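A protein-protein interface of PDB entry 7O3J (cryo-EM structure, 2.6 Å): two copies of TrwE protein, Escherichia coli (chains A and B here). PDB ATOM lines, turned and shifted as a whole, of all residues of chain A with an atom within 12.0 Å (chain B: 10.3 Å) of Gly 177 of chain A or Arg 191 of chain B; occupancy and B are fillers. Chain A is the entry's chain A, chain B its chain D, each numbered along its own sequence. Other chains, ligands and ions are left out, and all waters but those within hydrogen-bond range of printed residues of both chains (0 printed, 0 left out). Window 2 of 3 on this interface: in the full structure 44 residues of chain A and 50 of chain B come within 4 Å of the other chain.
The backbone carbonyl oxygen of Pro 189 of chain B sits at hydrogen-bond distance from the backbone NH of Gly 179 of chain A (2.9 Å).
Among the printed residues, pairs that only touch across the chains: Gly 177 of chain A with Pro 189 of chain B (3.3 Å), Gly 177 of chain A with Arg 191 of chain B (3.5 Å), Gly 178 of chain A with Pro 189 of chain B (3.5 Å), Gly 179 of chain A with Gln 188 of chain B (3.7 Å), Gly 179 of chain A with Met 190 of chain B (3.6 Å), Leu 183 of chain A with Met 190 of chain B (3.8 Å), Ala 184 of chain A with Met 190 of chain B (3.999 Å) and Leu 187 of chain A with Leu 192 of chain B (3.997 Å).
Of chain A, only Gly 177 (3.5 Å) comes within 4 Å of Arg 191 of chain B.
Gly 179 of chain A touches three residues of chain B.
Ser 193 of chain B touches none of the printed residues of chain A.
Printed residues of chain B within 4 Å of Ala 184 of chain A: Met 190.
Printed residues of chain A within 4 Å of Gln 188 of chain B: Gly 179 (3.7 Å).
Of the printed residues of chain B, Leu 183 of chain A touches Met 190 (3.8 Å).
Printed residues of chain B within 4 Å of Leu 187 of chain A: Leu 192.
Of the printed residues of chain A, Met 190 of chain B touches Gly 179, Leu 183 and Ala 184.
Pro 189 of chain A touches none of the printed residues of chain B.
The nearest residue of chain B that does not touch Gly 177 of chain A is Met 190 of chain B (4.6 Å).
Of the 10 printed residues of chain B, 5 touch a printed residue of chain A.
Hydrophobic or aromatic side chains of chain B within 4 Å of the printed part of chain A: Pro 189, Met 190 and Leu 192.
Hydrophobic or aromatic side chains of chain A that line the printed part of chain B: Leu 183, Ala 184 and Leu 187.
Among the printed residues, 9 pairs touch across the chains.
Among the printed residues, no Asp or Glu carboxylate lies within 4 Å of a Lys or Arg side-chain nitrogen of the other chain.
Positions printed for both chains: 184, 185, 187, 188 and 189.
Of the 9 pairs that touch across the chains among the printed residues, none has its exchanged pair printed and touching as well.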
ATOM      1  N   GLY A 177     -10.807  -5.987 -22.045  1.00  0.00           N
ATOM      2  CA  GLY A 177     -12.142  -5.564 -21.677  1.00  0.00           C
ATOM      3  C   GLY A 177     -12.554  -4.333 -22.449  1.00  0.00           C
ATOM      4  O   GLY A 177     -11.714  -3.571 -22.937  1.00  0.00           O
ATOM      5  N   GLY A 178     -13.868  -4.155 -22.556  1.00  0.00           N
ATOM      6  CA  GLY A 178     -14.430  -3.020 -23.258  1.00  0.00           C
ATOM      7  C   GLY A 178     -15.179  -2.070 -22.349  1.00  0.00           C
ATOM      8  O   GLY A 178     -16.003  -1.277 -22.812  1.00  0.00           O
ATOM      9  N   GLY A 179     -14.901  -2.140 -21.052  1.00  0.00           N
ATOM     10  CA  GLY A 179     -15.584  -1.311 -20.086  1.00  0.00           C
ATOM     11  C   GLY A 179     -15.039   0.103 -20.044  1.00  0.00           C
ATOM     12  O   GLY A 179     -14.231   0.530 -20.869  1.00  0.00           O
ATOM     13  N   GLY A 180     -15.502   0.847 -19.043  1.00  0.00           N
ATOM     14  CA  GLY A 180     -15.126   2.239 -18.899  1.00  0.00           C
ATOM     15  C   GLY A 180     -15.580   3.084 -20.068  1.00  0.00           C
ATOM     16  O   GLY A 180     -14.807   3.893 -20.583  1.00  0.00           O
ATOM     17  N   GLY A 181     -16.844   2.924 -20.467  1.00  0.00           N
ATOM     18  CA  GLY A 181     -17.282   3.408 -21.769  1.00  0.00           C
ATOM     19  C   GLY A 181     -17.081   4.897 -21.970  1.00  0.00           C
ATOM     20  O   GLY A 181     -16.586   5.329 -23.010  1.00  0.00           O
ATOM     21  N   GLU A 182     -17.469   5.703 -20.983  1.00  0.00           N
ATOM     22  CA  GLU A 182     -17.349   7.150 -21.130  1.00  0.00           C
ATOM     23  C   GLU A 182     -15.892   7.592 -21.125  1.00  0.00           C
ATOM     24  O   GLU A 182     -15.458   8.364 -21.991  1.00  0.00           O
ATOM     25  CB  GLU A 182     -18.124   7.851 -20.019  1.00  0.00           C
ATOM     26  CG  GLU A 182     -18.460   9.286 -20.333  1.00  0.00           C
ATOM     27  CD  GLU A 182     -18.743  10.106 -19.097  1.00  0.00           C
ATOM     28  OE1 GLU A 182     -18.890   9.514 -18.010  1.00  0.00           O
ATOM     29  OE2 GLU A 182     -18.824  11.345 -19.217  1.00  0.00           O
ATOM     30  N   LEU A 183     -15.118   7.108 -20.158  1.00  0.00           N
ATOM     31  CA  LEU A 183     -13.716   7.486 -20.077  1.00  0.00           C
ATOM     32  C   LEU A 183     -12.929   6.925 -21.250  1.00  0.00           C
ATOM     33  O   LEU A 183     -11.986   7.560 -21.731  1.00  0.00           O
ATOM     34  CB  LEU A 183     -13.126   7.014 -18.753  1.00  0.00           C
ATOM     35  CG  LEU A 183     -11.678   7.392 -18.471  1.00  0.00           C
ATOM     36  CD1 LEU A 183     -11.475   8.876 -18.601  1.00  0.00           C
ATOM     37  CD2 LEU A 183     -11.307   6.932 -17.103  1.00  0.00           C
ATOM     38  N   ALA A 184     -13.295   5.736 -21.725  1.00  0.00           N
ATOM     39  CA  ALA A 184     -12.566   5.142 -22.837  1.00  0.00           C
ATOM     40  C   ALA A 184     -12.868   5.844 -24.150  1.00  0.00           C
ATOM     41  O   ALA A 184     -12.043   5.805 -25.068  1.00  0.00           O
ATOM     42  CB  ALA A 184     -12.887   3.657 -22.955  1.00  0.00           C
ATOM     43  N   GLU A 185     -14.036   6.473 -24.272  1.00  0.00           N
ATOM     44  CA  GLU A 185     -14.332   7.205 -25.492  1.00  0.00           C
ATOM     45  C   GLU A 185     -13.856   8.646 -25.430  1.00  0.00           C
ATOM     46  O   GLU A 185     -13.665   9.261 -26.481  1.00  0.00           O
ATOM     47  CB  GLU A 185     -15.827   7.164 -25.807  1.00  0.00           C
ATOM     48  CG  GLU A 185     -16.713   7.876 -24.814  1.00  0.00           C
ATOM     49  CD  GLU A 185     -18.186   7.735 -25.152  1.00  0.00           C
ATOM     50  OE1 GLU A 185     -18.502   7.060 -26.152  1.00  0.00           O
ATOM     51  OE2 GLU A 185     -19.026   8.298 -24.419  1.00  0.00           O
ATOM     52  N   LEU A 187     -10.901   9.138 -24.313  1.00  0.00           N
ATOM     53  CA  LEU A 187      -9.475   8.936 -24.499  1.00  0.00           C
ATOM     54  C   LEU A 187      -9.131   8.408 -25.882  1.00  0.00           C
ATOM     55  O   LEU A 187      -7.993   7.987 -26.102  1.00  0.00           O
ATOM     56  CB  LEU A 187      -8.929   7.993 -23.432  1.00  0.00           C
ATOM     57  CG  LEU A 187      -8.794   8.606 -22.044  1.00  0.00           C
ATOM     58  CD1 LEU A 187      -8.267   7.588 -21.073  1.00  0.00           C
ATOM     59  CD2 LEU A 187      -7.905   9.817 -22.087  1.00  0.00           C
ATOM     60  N   GLN A 188     -10.074   8.413 -26.807  1.00  0.00           N
ATOM     61  CA  GLN A 188      -9.774   8.025 -28.176  1.00  0.00           C
ATOM     62  C   GLN A 188      -8.884   9.078 -28.819  1.00  0.00           C
ATOM     63  O   GLN A 188      -9.228  10.264 -28.803  1.00  0.00           O
ATOM     64  CB  GLN A 188     -11.049   7.860 -28.984  1.00  0.00           C
ATOM     65  CG  GLN A 188     -11.911   6.711 -28.544  1.00  0.00           C
ATOM     66  CD  GLN A 188     -13.174   6.601 -29.362  1.00  0.00           C
ATOM     67  OE1 GLN A 188     -13.437   7.434 -30.226  1.00  0.00           O
ATOM     68  NE2 GLN A 188     -13.970   5.573 -29.091  1.00  0.00           N
ATOM     69  N   PRO A 189      -7.749   8.695 -29.389  1.00  0.00           N
ATOM     70  CA  PRO A 189      -6.812   9.689 -29.914  1.00  0.00           C
ATOM     71  C   PRO A 189      -7.340  10.379 -31.156  1.00  0.00           C
ATOM     72  O   PRO A 189      -8.158   9.840 -31.904  1.00  0.00           O
ATOM     73  CB  PRO A 189      -5.570   8.858 -30.238  1.00  0.00           C
ATOM     74  CG  PRO A 189      -6.076   7.504 -30.474  1.00  0.00           C
ATOM     75  CD  PRO A 189      -7.302   7.320 -29.647  1.00  0.00           C
ATOM     76  N   ALA B 184     -21.703  -6.546 -12.192  1.00  0.00           N
ATOM     77  CA  ALA B 184     -20.811  -7.201 -13.140  1.00  0.00           C
ATOM     78  C   ALA B 184     -20.484  -6.305 -14.320  1.00  0.00           C
ATOM     79  O   ALA B 184     -19.438  -6.481 -14.951  1.00  0.00           O
ATOM     80  CB  ALA B 184     -21.421  -8.510 -13.631  1.00  0.00           C
ATOM     81  N   GLU B 185     -21.360  -5.356 -14.649  1.00  0.00           N
ATOM     82  CA  GLU B 185     -21.051  -4.441 -15.736  1.00  0.00           C
ATOM     83  C   GLU B 185     -20.294  -3.215 -15.261  1.00  0.00           C
ATOM     84  O   GLU B 185     -19.624  -2.571 -16.070  1.00  0.00           O
ATOM     85  CB  GLU B 185     -22.321  -4.014 -16.470  1.00  0.00           C
ATOM     86  CG  GLU B 185     -23.290  -3.189 -15.657  1.00  0.00           C
ATOM     87  CD  GLU B 185     -24.555  -2.862 -16.425  1.00  0.00           C
ATOM     88  OE1 GLU B 185     -24.675  -3.304 -17.586  1.00  0.00           O
ATOM     89  OE2 GLU B 185     -25.431  -2.163 -15.872  1.00  0.00           O
ATOM     90  N   LEU B 187     -17.848  -3.721 -13.265  1.00  0.00           N
ATOM     91  CA  LEU B 187     -16.531  -4.307 -13.068  1.00  0.00           C
ATOM     92  C   LEU B 187     -15.886  -4.757 -14.367  1.00  0.00           C
ATOM     93  O   LEU B 187     -14.876  -5.461 -14.327  1.00  0.00           O
ATOM     94  CB  LEU B 187     -16.612  -5.476 -12.093  1.00  0.00           C
ATOM     95  CG  LEU B 187     -16.802  -5.083 -10.633  1.00  0.00           C
ATOM     96  CD1 LEU B 187     -16.884  -6.309  -9.769  1.00  0.00           C
ATOM     97  CD2 LEU B 187     -15.685  -4.183 -10.182  1.00  0.00           C
ATOM     98  N   GLN B 188     -16.442  -4.379 -15.505  1.00  0.00           N
ATOM     99  CA  GLN B 188     -15.807  -4.686 -16.777  1.00  0.00           C
ATOM    100  C   GLN B 188     -14.529  -3.871 -16.918  1.00  0.00           C
ATOM    101  O   GLN B 188     -14.566  -2.646 -16.772  1.00  0.00           O
ATOM    102  CB  GLN B 188     -16.743  -4.387 -17.935  1.00  0.00           C
ATOM    103  CG  GLN B 188     -17.951  -5.279 -17.995  1.00  0.00           C
ATOM    104  CD  GLN B 188     -18.860  -4.930 -19.147  1.00  0.00           C
ATOM    105  OE1 GLN B 188     -18.615  -3.967 -19.872  1.00  0.00           O
ATOM    106  NE2 GLN B 188     -19.922  -5.707 -19.323  1.00  0.00           N
ATOM    107  N   PRO B 189     -13.397  -4.501 -17.199  1.00  0.00           N
ATOM    108  CA  PRO B 189     -12.131  -3.770 -17.228  1.00  0.00           C
ATOM    109  C   PRO B 189     -12.036  -2.827 -18.411  1.00  0.00           C
ATOM    110  O   PRO B 189     -12.664  -3.019 -19.452  1.00  0.00           O
ATOM    111  CB  PRO B 189     -11.088  -4.884 -17.336  1.00  0.00           C
ATOM    112  CG  PRO B 189     -11.795  -5.998 -17.967  1.00  0.00           C
ATOM    113  CD  PRO B 189     -13.232  -5.911 -17.581  1.00  0.00           C
ATOM    114  N   MET B 190     -11.239  -1.785 -18.229  1.00  0.00           N
ATOM    115  CA  MET B 190     -10.868  -0.884 -19.309  1.00  0.00           C
ATOM    116  C   MET B 190      -9.384  -1.101 -19.567  1.00  0.00           C
ATOM    117  O   MET B 190      -8.544  -0.702 -18.756  1.00  0.00           O
ATOM    118  CB  MET B 190     -11.165   0.566 -18.944  1.00  0.00           C
ATOM    119  CG  MET B 190     -10.521   1.572 -19.864  1.00  0.00           C
ATOM    120  SD  MET B 190     -10.977   3.259 -19.464  1.00  0.00           S
ATOM    121  CE  MET B 190      -9.944   3.525 -18.039  1.00  0.00           C
ATOM    122  N   ARG B 191      -9.064  -1.751 -20.678  1.00  0.00           N
ATOM    123  CA  ARG B 191      -7.694  -2.111 -21.012  1.00  0.00           C
ATOM    124  C   ARG B 191      -7.221  -1.194 -22.128  1.00  0.00           C
ATOM    125  O   ARG B 191      -7.721  -1.270 -23.254  1.00  0.00           O
ATOM    126  CB  ARG B 191      -7.601  -3.576 -21.427  1.00  0.00           C
ATOM    127  CG  ARG B 191      -8.132  -4.538 -20.393  1.00  0.00           C
ATOM    128  CD  ARG B 191      -7.089  -4.870 -19.352  1.00  0.00           C
ATOM    129  NE  ARG B 191      -7.689  -5.486 -18.178  1.00  0.00           N
ATOM    130  CZ  ARG B 191      -7.945  -6.784 -18.063  1.00  0.00           C
ATOM    131  NH1 ARG B 191      -7.652  -7.610 -19.054  1.00  0.00           N
ATOM    132  NH2 ARG B 191      -8.496  -7.259 -16.957  1.00  0.00           N
ATOM    133  N   LEU B 192      -6.259  -0.337 -21.817  1.00  0.00           N
ATOM    134  CA  LEU B 192      -5.727   0.622 -22.772  1.00  0.00           C
ATOM    135  C   LEU B 192      -4.381   0.132 -23.279  1.00  0.00           C
ATOM    136  O   LEU B 192      -3.499  -0.209 -22.486  1.00  0.00           O
ATOM    137  CB  LEU B 192      -5.593   2.001 -22.132  1.00  0.00           C
ATOM    138  CG  LEU B 192      -6.894   2.621 -21.626  1.00  0.00           C
ATOM    139  CD1 LEU B 192      -6.627   3.945 -20.965  1.00  0.00           C
ATOM    140  CD2 LEU B 192      -7.880   2.787 -22.755  1.00  0.00           C
ATOM    141  N   SER B 193      -4.233   0.094 -24.598  1.00  0.00           N
ATOM    142  CA  SER B 193      -3.012  -0.405 -25.208  1.00  0.00           C
ATOM    143  C   SER B 193      -1.845   0.525 -24.915  1.00  0.00           C
ATOM    144  O   SER B 193      -1.991   1.747 -24.919  1.00  0.00           O
ATOM    145  CB  SER B 193      -3.200  -0.540 -26.716  1.00  0.00           C
ATOM    146  OG  SER B 193      -4.210  -1.482 -27.016  1.00  0.00           O
ATOM    147  N   GLY B 194      -0.680  -0.060 -24.674  1.00  0.00           N
ATOM    148  CA  GLY B 194       0.507   0.725 -24.425  1.00  0.00           C
ATOM    149  C   GLY B 194       1.034   1.378 -25.684  1.00  0.00           C
ATOM    150  O   GLY B 194       0.588   1.119 -26.799  1.00  0.00           O
